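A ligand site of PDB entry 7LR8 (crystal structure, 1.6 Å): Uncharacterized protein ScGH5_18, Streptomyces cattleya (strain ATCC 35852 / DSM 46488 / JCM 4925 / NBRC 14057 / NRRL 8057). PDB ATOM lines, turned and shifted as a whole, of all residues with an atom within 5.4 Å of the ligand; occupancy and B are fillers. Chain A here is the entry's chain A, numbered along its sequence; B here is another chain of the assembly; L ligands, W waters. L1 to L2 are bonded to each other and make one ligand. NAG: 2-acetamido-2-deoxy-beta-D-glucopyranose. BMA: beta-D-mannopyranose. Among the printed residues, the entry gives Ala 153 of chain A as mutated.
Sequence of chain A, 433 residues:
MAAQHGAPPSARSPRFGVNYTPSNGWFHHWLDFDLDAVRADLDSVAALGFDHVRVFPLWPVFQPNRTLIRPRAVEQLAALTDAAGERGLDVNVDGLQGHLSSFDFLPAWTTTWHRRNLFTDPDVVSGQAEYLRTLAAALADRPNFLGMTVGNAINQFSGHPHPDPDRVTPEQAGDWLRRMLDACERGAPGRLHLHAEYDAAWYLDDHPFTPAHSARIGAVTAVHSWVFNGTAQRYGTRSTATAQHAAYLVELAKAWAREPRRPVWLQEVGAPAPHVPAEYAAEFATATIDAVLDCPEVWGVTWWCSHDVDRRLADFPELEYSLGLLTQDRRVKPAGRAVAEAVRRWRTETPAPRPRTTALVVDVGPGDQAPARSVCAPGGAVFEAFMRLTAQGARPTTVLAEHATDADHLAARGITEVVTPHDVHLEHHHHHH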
ATOM      1  N   HIS A  99       1.641 -16.954 -23.246  1.00  0.00           N
ATOM      2  CA  HIS A  99       1.437 -15.978 -24.306  1.00  0.00           C
ATOM      3  C   HIS A  99       2.159 -16.382 -25.587  1.00  0.00           C
ATOM      4  O   HIS A  99       3.365 -16.648 -25.574  1.00  0.00           O
ATOM      5  CB  HIS A  99       1.920 -14.585 -23.887  1.00  0.00           C
ATOM      6  CG  HIS A  99       1.624 -13.552 -24.924  1.00  0.00           C
ATOM      7  ND1 HIS A  99       0.390 -12.954 -25.025  1.00  0.00           N
ATOM      8  CD2 HIS A  99       2.373 -13.081 -25.956  1.00  0.00           C
ATOM      9  CE1 HIS A  99       0.394 -12.127 -26.054  1.00  0.00           C
ATOM     10  NE2 HIS A  99       1.580 -12.185 -26.645  1.00  0.00           N
ATOM     11  N   LEU A 100       1.409 -16.399 -26.702  1.00  0.00           N
ATOM     12  CA  LEU A 100       2.008 -16.579 -28.018  1.00  0.00           C
ATOM     13  C   LEU A 100       1.333 -15.656 -29.017  1.00  0.00           C
ATOM     14  O   LEU A 100       0.132 -15.793 -29.282  1.00  0.00           O
ATOM     15  CB  LEU A 100       1.888 -18.027 -28.486  1.00  0.00           C
ATOM     16  CG  LEU A 100       2.766 -19.042 -27.732  1.00  0.00           C
ATOM     17  CD1 LEU A 100       2.221 -20.444 -27.956  1.00  0.00           C
ATOM     18  CD2 LEU A 100       4.218 -18.964 -28.206  1.00  0.00           C
ATOM     19  N   SER A 101       2.099 -14.702 -29.562  1.00  0.00           N
ATOM     20  CA  SER A 101       1.737 -13.970 -30.792  1.00  0.00           C
ATOM     21  C   SER A 101       0.403 -13.231 -30.656  1.00  0.00           C
ATOM     22  O   SER A 101      -0.417 -13.246 -31.586  1.00  0.00           O
ATOM     23  CB  SER A 101       1.682 -14.939 -31.984  1.00  0.00           C
ATOM     24  OG  SER A 101       2.881 -15.674 -32.097  1.00  0.00           O
ATOM     25  N   SER A 102       0.192 -12.599 -29.499  1.00  0.00           N
ATOM     26  CA  SER A 102      -0.935 -11.740 -29.107  1.00  0.00           C
ATOM     27  C   SER A 102      -2.028 -12.502 -28.369  1.00  0.00           C
ATOM     28  O   SER A 102      -2.922 -11.859 -27.828  1.00  0.00           O
ATOM     29  CB  SER A 102      -1.589 -10.981 -30.285  1.00  0.00           C
ATOM     30  OG  SER A 102      -2.490 -11.809 -31.013  1.00  0.00           O
ATOM     31  N   ASN A 152       7.470 -18.551 -22.414  1.00  0.00           N
ATOM     32  CA  ASN A 152       7.800 -17.543 -23.413  1.00  0.00           C
ATOM     33  C   ASN A 152       7.318 -16.175 -22.936  1.00  0.00           C
ATOM     34  O   ASN A 152       6.145 -15.838 -23.064  1.00  0.00           O
ATOM     35  CB  ASN A 152       7.158 -17.910 -24.755  1.00  0.00           C
ATOM     36  CG  ASN A 152       7.299 -16.809 -25.793  1.00  0.00           C
ATOM     37  OD1 ASN A 152       6.456 -16.646 -26.662  1.00  0.00           O
ATOM     38  ND2 ASN A 152       8.370 -16.011 -25.676  1.00  0.00           N
ATOM     39  N   ALA A 153       8.232 -15.375 -22.381  1.00  0.00           N
ATOM     40  CA  ALA A 153       7.906 -14.029 -21.935  1.00  0.00           C
ATOM     41  C   ALA A 153       6.705 -14.053 -20.994  1.00  0.00           C
ATOM     42  O   ALA A 153       5.759 -13.267 -21.116  1.00  0.00           O
ATOM     43  CB  ALA A 153       7.659 -13.092 -23.112  1.00  0.00           C
ATOM     44  N   GLN A 156       4.920 -10.997 -19.414  1.00  0.00           N
ATOM     45  CA  GLN A 156       3.883 -10.124 -19.947  1.00  0.00           C
ATOM     46  C   GLN A 156       2.552 -10.250 -19.191  1.00  0.00           C
ATOM     47  O   GLN A 156       1.667  -9.415 -19.369  1.00  0.00           O
ATOM     48  CB  GLN A 156       3.673 -10.400 -21.442  1.00  0.00           C
ATOM     49  CG  GLN A 156       2.979 -11.716 -21.724  1.00  0.00           C
ATOM     50  CD  GLN A 156       1.512 -11.532 -22.054  1.00  0.00           C
ATOM     51  OE1 GLN A 156       1.148 -10.607 -22.754  1.00  0.00           O
ATOM     52  NE2 GLN A 156       0.660 -12.394 -21.509  1.00  0.00           N
ATOM     53  N   TYR A 198      10.378 -10.755 -21.961  1.00  0.00           N
ATOM     54  CA  TYR A 198      10.387  -9.748 -23.012  1.00  0.00           C
ATOM     55  C   TYR A 198      10.893  -8.398 -22.457  1.00  0.00           C
ATOM     56  O   TYR A 198      11.110  -8.240 -21.259  1.00  0.00           O
ATOM     57  CB  TYR A 198       8.998  -9.642 -23.675  1.00  0.00           C
ATOM     58  CG  TYR A 198       8.054  -8.575 -23.151  1.00  0.00           C
ATOM     59  CD1 TYR A 198       7.352  -8.753 -21.961  1.00  0.00           C
ATOM     60  CD2 TYR A 198       7.823  -7.407 -23.875  1.00  0.00           C
ATOM     61  CE1 TYR A 198       6.470  -7.798 -21.500  1.00  0.00           C
ATOM     62  CE2 TYR A 198       6.952  -6.420 -23.415  1.00  0.00           C
ATOM     63  CZ  TYR A 198       6.285  -6.621 -22.226  1.00  0.00           C
ATOM     64  OH  TYR A 198       5.399  -5.646 -21.780  1.00  0.00           O
ATOM     65  N   ASP A 199      11.095  -7.426 -23.358  1.00  0.00           N
ATOM     66  CA  ASP A 199      11.946  -6.276 -23.038  1.00  0.00           C
ATOM     67  C   ASP A 199      11.368  -5.328 -21.996  1.00  0.00           C
ATOM     68  O   ASP A 199      12.088  -4.423 -21.561  1.00  0.00           O
ATOM     69  CB  ASP A 199      12.317  -5.495 -24.327  1.00  0.00           C
ATOM     70  CG  ASP A 199      11.123  -4.954 -25.091  1.00  0.00           C
ATOM     71  OD1 ASP A 199      10.092  -4.614 -24.475  1.00  0.00           O
ATOM     72  OD2 ASP A 199      11.230  -4.849 -26.346  1.00  0.00           O
ATOM     73  N   HIS A 224      15.057 -11.014 -26.103  1.00  0.00           N
ATOM     74  CA  HIS A 224      14.119 -11.100 -27.219  1.00  0.00           C
ATOM     75  C   HIS A 224      14.096  -9.715 -27.837  1.00  0.00           C
ATOM     76  O   HIS A 224      13.649  -8.754 -27.189  1.00  0.00           O
ATOM     77  CB  HIS A 224      12.712 -11.518 -26.746  1.00  0.00           C
ATOM     78  CG  HIS A 224      12.632 -12.900 -26.167  1.00  0.00           C
ATOM     79  ND1 HIS A 224      11.582 -13.313 -25.385  1.00  0.00           N
ATOM     80  CD2 HIS A 224      13.482 -13.957 -26.241  1.00  0.00           C
ATOM     81  CE1 HIS A 224      11.772 -14.572 -25.010  1.00  0.00           C
ATOM     82  NE2 HIS A 224      12.914 -14.984 -25.517  1.00  0.00           N
ATOM     83  N   TRP A 226      13.009  -6.947 -30.548  1.00  0.00           N
ATOM     84  CA  TRP A 226      11.849  -6.627 -31.393  1.00  0.00           C
ATOM     85  C   TRP A 226      11.794  -5.121 -31.642  1.00  0.00           C
ATOM     86  O   TRP A 226      11.428  -4.359 -30.748  1.00  0.00           O
ATOM     87  CB  TRP A 226      10.581  -7.157 -30.711  1.00  0.00           C
ATOM     88  CG  TRP A 226      10.509  -8.668 -30.797  1.00  0.00           C
ATOM     89  CD1 TRP A 226      10.731  -9.573 -29.775  1.00  0.00           C
ATOM     90  CD2 TRP A 226      10.240  -9.432 -31.972  1.00  0.00           C
ATOM     91  NE1 TRP A 226      10.594 -10.852 -30.262  1.00  0.00           N
ATOM     92  CE2 TRP A 226      10.292 -10.792 -31.606  1.00  0.00           C
ATOM     93  CE3 TRP A 226       9.973  -9.101 -33.306  1.00  0.00           C
ATOM     94  CZ2 TRP A 226      10.065 -11.826 -32.520  1.00  0.00           C
ATOM     95  CZ3 TRP A 226       9.721 -10.132 -34.220  1.00  0.00           C
ATOM     96  CH2 TRP A 226       9.781 -11.465 -33.817  1.00  0.00           C
ATOM     97  N   PHE A 228       9.831  -3.222 -33.218  1.00  0.00           N
ATOM     98  CA  PHE A 228       8.564  -2.513 -33.087  1.00  0.00           C
ATOM     99  C   PHE A 228       8.335  -1.960 -31.671  1.00  0.00           C
ATOM    100  O   PHE A 228       7.276  -1.395 -31.406  1.00  0.00           O
ATOM    101  CB  PHE A 228       7.375  -3.403 -33.500  1.00  0.00           C
ATOM    102  CG  PHE A 228       7.238  -4.730 -32.744  1.00  0.00           C
ATOM    103  CD1 PHE A 228       7.179  -4.800 -31.350  1.00  0.00           C
ATOM    104  CD2 PHE A 228       7.076  -5.913 -33.460  1.00  0.00           C
ATOM    105  CE1 PHE A 228       7.021  -6.028 -30.698  1.00  0.00           C
ATOM    106  CE2 PHE A 228       6.906  -7.138 -32.815  1.00  0.00           C
ATOM    107  CZ  PHE A 228       6.881  -7.195 -31.429  1.00  0.00           C
ATOM    108  N   GLU A 268      15.083 -14.654 -29.360  1.00  0.00           N
ATOM    109  CA  GLU A 268      14.166 -14.200 -30.397  1.00  0.00           C
ATOM    110  C   GLU A 268      14.768 -12.995 -31.090  1.00  0.00           C
ATOM    111  O   GLU A 268      15.289 -12.081 -30.438  1.00  0.00           O
ATOM    112  CB  GLU A 268      12.788 -13.817 -29.854  1.00  0.00           C
ATOM    113  CG  GLU A 268      12.024 -14.945 -29.199  1.00  0.00           C
ATOM    114  CD  GLU A 268      10.690 -14.494 -28.648  1.00  0.00           C
ATOM    115  OE1 GLU A 268      10.325 -13.314 -28.844  1.00  0.00           O
ATOM    116  OE2 GLU A 268      10.017 -15.317 -27.976  1.00  0.00           O
ATOM    117  N   TRP A 304      12.884 -15.646 -34.961  1.00  0.00           N
ATOM    118  CA  TRP A 304      11.430 -15.755 -34.940  1.00  0.00           C
ATOM    119  C   TRP A 304      10.887 -15.341 -36.312  1.00  0.00           C
ATOM    120  O   TRP A 304      10.848 -14.152 -36.622  1.00  0.00           O
ATOM    121  CB  TRP A 304      10.814 -14.874 -33.852  1.00  0.00           C
ATOM    122  CG  TRP A 304       9.350 -15.204 -33.727  1.00  0.00           C
ATOM    123  CD1 TRP A 304       8.357 -14.862 -34.605  1.00  0.00           C
ATOM    124  CD2 TRP A 304       8.722 -15.995 -32.716  1.00  0.00           C
ATOM    125  NE1 TRP A 304       7.151 -15.395 -34.209  1.00  0.00           N
ATOM    126  CE2 TRP A 304       7.346 -16.096 -33.037  1.00  0.00           C
ATOM    127  CE3 TRP A 304       9.182 -16.628 -31.549  1.00  0.00           C
ATOM    128  CZ2 TRP A 304       6.430 -16.793 -32.245  1.00  0.00           C
ATOM    129  CZ3 TRP A 304       8.273 -17.331 -30.759  1.00  0.00           C
ATOM    130  CH2 TRP A 304       6.912 -17.403 -31.106  1.00  0.00           C
ATOM    131  N   PRO A 317      -2.557  -9.986 -35.157  1.00  0.00           N
ATOM    132  CA  PRO A 317      -1.997  -8.741 -35.710  1.00  0.00           C
ATOM    133  C   PRO A 317      -1.286  -9.085 -37.011  1.00  0.00           C
ATOM    134  O   PRO A 317      -0.597 -10.099 -37.115  1.00  0.00           O
ATOM    135  CB  PRO A 317      -1.027  -8.268 -34.633  1.00  0.00           C
ATOM    136  CG  PRO A 317      -1.569  -8.855 -33.371  1.00  0.00           C
ATOM    137  CD  PRO A 317      -2.137 -10.203 -33.756  1.00  0.00           C
ATOM    138  N   LEU A 319       1.321  -8.224 -38.444  1.00  0.00           N
ATOM    139  CA  LEU A 319       2.757  -8.479 -38.438  1.00  0.00           C
ATOM    140  C   LEU A 319       3.079  -9.952 -38.184  1.00  0.00           C
ATOM    141  O   LEU A 319       4.099 -10.444 -38.666  1.00  0.00           O
ATOM    142  CB  LEU A 319       3.446  -7.581 -37.397  1.00  0.00           C
ATOM    143  CG  LEU A 319       3.243  -7.982 -35.917  1.00  0.00           C
ATOM    144  CD1 LEU A 319       4.377  -8.875 -35.406  1.00  0.00           C
ATOM    145  CD2 LEU A 319       3.083  -6.737 -35.049  1.00  0.00           C
ATOM    146  N   GLU A 320       2.234 -10.660 -37.427  1.00  0.00           N
ATOM    147  CA  GLU A 320       2.568 -12.029 -37.066  1.00  0.00           C
ATOM    148  C   GLU A 320       2.616 -12.943 -38.279  1.00  0.00           C
ATOM    149  O   GLU A 320       3.381 -13.915 -38.294  1.00  0.00           O
ATOM    150  CB  GLU A 320       1.572 -12.589 -36.046  1.00  0.00           C
ATOM    151  CG  GLU A 320       1.544 -11.796 -34.724  1.00  0.00           C
ATOM    152  CD  GLU A 320       2.771 -12.015 -33.835  1.00  0.00           C
ATOM    153  OE1 GLU A 320       3.617 -12.884 -34.136  1.00  0.00           O
ATOM    154  OE2 GLU A 320       2.858 -11.323 -32.801  1.00  0.00           O
ATOM    155  N   LEU A 323       6.271 -13.328 -40.327  1.00  0.00           N
ATOM    156  CA  LEU A 323       7.530 -13.394 -39.594  1.00  0.00           C
ATOM    157  C   LEU A 323       8.364 -14.627 -39.929  1.00  0.00           C
ATOM    158  O   LEU A 323       9.486 -14.742 -39.413  1.00  0.00           O
ATOM    159  CB  LEU A 323       7.256 -13.333 -38.084  1.00  0.00           C
ATOM    160  CG  LEU A 323       6.912 -11.956 -37.532  1.00  0.00           C
ATOM    161  CD1 LEU A 323       6.605 -12.033 -36.029  1.00  0.00           C
ATOM    162  CD2 LEU A 323       8.026 -10.915 -37.794  1.00  0.00           C
ATOM    163  N   TRP B 113      -6.043  -9.817 -24.483  1.00  0.00           N
ATOM    164  CA  TRP B 113      -5.691  -8.970 -25.628  1.00  0.00           C
ATOM    165  C   TRP B 113      -6.769  -8.984 -26.700  1.00  0.00           C
ATOM    166  O   TRP B 113      -6.831  -8.048 -27.513  1.00  0.00           O
ATOM    167  CB  TRP B 113      -4.369  -9.410 -26.244  1.00  0.00           C
ATOM    168  CG  TRP B 113      -3.208  -9.383 -25.310  1.00  0.00           C
ATOM    169  CD1 TRP B 113      -2.615 -10.462 -24.704  1.00  0.00           C
ATOM    170  CD2 TRP B 113      -2.497  -8.230 -24.860  1.00  0.00           C
ATOM    171  NE1 TRP B 113      -1.559 -10.039 -23.925  1.00  0.00           N
ATOM    172  CE2 TRP B 113      -1.480  -8.670 -23.993  1.00  0.00           C
ATOM    173  CE3 TRP B 113      -2.619  -6.854 -25.114  1.00  0.00           C
ATOM    174  CZ2 TRP B 113      -0.582  -7.794 -23.390  1.00  0.00           C
ATOM    175  CZ3 TRP B 113      -1.726  -5.986 -24.506  1.00  0.00           C
ATOM    176  CH2 TRP B 113      -0.729  -6.461 -23.655  1.00  0.00           C
HETATM  177  C1  NAG L   1       4.687  -7.897 -27.439  1.00  0.00           C
HETATM  178  C2  NAG L   1       3.717  -8.933 -28.035  1.00  0.00           C
HETATM  179  C3  NAG L   1       4.293 -10.344 -27.882  1.00  0.00           C
HETATM  180  C4  NAG L   1       5.729 -10.420 -28.392  1.00  0.00           C
HETATM  181  C5  NAG L   1       6.551  -9.329 -27.697  1.00  0.00           C
HETATM  182  C6  NAG L   1       7.992  -9.253 -28.118  1.00  0.00           C
HETATM  183  C7  NAG L   1       1.244  -8.851 -28.003  1.00  0.00           C
HETATM  184  C8  NAG L   1       0.027  -8.713 -27.139  1.00  0.00           C
HETATM  185  N2  NAG L   1       2.423  -8.823 -27.378  1.00  0.00           N
HETATM  186  O1  NAG L   1       4.201  -6.613 -27.654  1.00  0.00           O
HETATM  187  O3  NAG L   1       3.460 -11.296 -28.548  1.00  0.00           O
HETATM  188  O4  NAG L   1       6.247 -11.728 -28.141  1.00  0.00           O
HETATM  189  O5  NAG L   1       5.971  -8.056 -28.010  1.00  0.00           O
HETATM  190  O6  NAG L   1       8.699  -8.259 -27.374  1.00  0.00           O
HETATM  191  O7  NAG L   1       1.157  -8.986 -29.227  1.00  0.00           O
HETATM  192  C1  BMA L   2       7.244 -12.263 -29.073  1.00  0.00           C
HETATM  193  C2  BMA L   2       7.045 -13.798 -29.248  1.00  0.00           C
HETATM  194  C3  BMA L   2       5.662 -14.040 -29.854  1.00  0.00           C
HETATM  195  C4  BMA L   2       5.361 -13.025 -31.023  1.00  0.00           C
HETATM  196  C5  BMA L   2       6.619 -12.276 -31.463  1.00  0.00           C
HETATM  197  C6  BMA L   2       6.361 -11.217 -32.527  1.00  0.00           C
HETATM  198  O2  BMA L   2       7.106 -14.478 -27.977  1.00  0.00           O
HETATM  199  O3  BMA L   2       4.690 -13.949 -28.853  1.00  0.00           O
HETATM  200  O4  BMA L   2       4.848 -13.742 -32.128  1.00  0.00           O
HETATM  201  O5  BMA L   2       7.219 -11.554 -30.346  1.00  0.00           O
HETATM  202  O6  BMA L   2       5.428 -10.295 -32.019  1.00  0.00           O
HETATM  203  O   HOH W   1       1.547  -9.227 -31.629  1.00  0.00           O
HETATM  204  O   HOH W   2       1.490  -4.909 -26.537  1.00  0.00           O
HETATM  205  O   HOH W   3      11.015  -8.406 -26.042  1.00  0.00           O
HETATM  206  O   HOH W   4       3.658  -7.337 -31.484  1.00  0.00           O
HETATM  207  O   HOH W   5       6.207 -11.980 -25.607  1.00  0.00           O
HETATM  208  O   HOH W   6       5.310 -14.665 -25.514  1.00  0.00           O
HETATM  209  O   HOH W   7       2.707  -9.198 -24.683  1.00  0.00           O
HETATM  210  O   HOH W   8       8.996 -12.660 -26.317  1.00  0.00           O
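Residues that only touch the ligand: Leu 100 (3.8 Å), Ser 102 (3.5 Å), Tyr 198 (3.7 Å), Phe 228 (3.5 Å), Trp 304 (3.4 Å), Leu 319 (3.8 Å), Leu 323 (3.6 Å) and Trp 113 of chain B (3.4 Å). Hydrophobic or aromatic side chains that line the ligand: His 99, Tyr 198, Trp 226, Phe 228, Trp 304, Leu 319, Leu 323 and Trp 113 of chain B. The nearest printed residue that does not touch the ligand is Asp 199 (4.4 Å).
OE1 of Glu 320 sits at hydrogen-bond distance from O4 of BMA L2 (2.5 Å). The side-chain amide oxygen of Asn 152 lies within hydrogen-bond range of an oxygen (O2) of BMA L2. N of Ser 101 sits at hydrogen-bond distance from O3 of BMA L2 (2.8 Å). OG of Ser 101 lies within hydrogen-bond range of O4 of BMA L2, 2.8 Å away. A ring nitrogen (NE2) of His 99 sits at hydrogen-bond distance from an oxygen (O3) of NAG L1, at 2.8 Å. O2 of BMA L2 sits at hydrogen-bond distance from OE2 of Glu 268 (3.0 Å). The indole nitrogen of Trp 226 sits close to an oxygen (O5) of BMA L2 (3.4 Å).
OD1 of Asn 152 lies close to O of His 99. The side-chain amide nitrogen (ND2) of Asn 152 lies within hydrogen-bond range of the side-chain carboxylate (OE2) of Glu 268, at 2.9 Å. N of Ser 102 is in hydrogen-bond range of NE2 of His 99 (3.2 Å). A ring nitrogen (ND1) of His 99 lies within hydrogen-bond range of the side-chain amide oxygen of Gln 156 (3.4 Å). OE1 of Glu 268 sits at hydrogen-bond distance from NE1 of Trp 226 (2.9 Å). The side-chain amide oxygen of Gln 156 sits at hydrogen-bond distance from the indole nitrogen of Trp 113 of chain B, 3.0 Å away.
Water W1 bridges an oxygen (O7) of NAG L1 (2.4 Å) and the side-chain carboxylate (OE2) of Glu 320 (2.7 Å). Water W3 lies within hydrogen-bond range of O6 of NAG L1 (2.7 Å), N of Asp 199 (2.9 Å) and O of His 224 (2.9 Å). Water W7 lies within hydrogen-bond range of N2 of NAG L1 and OE1 of Gln 156. Water W6 lies within hydrogen-bond range of OD1 of Asn 152 (2.6 Å), O of His 99 (2.8 Å) and O2 of BMA L2 (3.1 Å). Water W8 lies within hydrogen-bond range of ND1 of His 224 (2.8 Å), OE1 of Glu 268 (2.9 Å), O2 of BMA L2 (3.1 Å) and ND2 of Asn 152 (3.5 Å).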
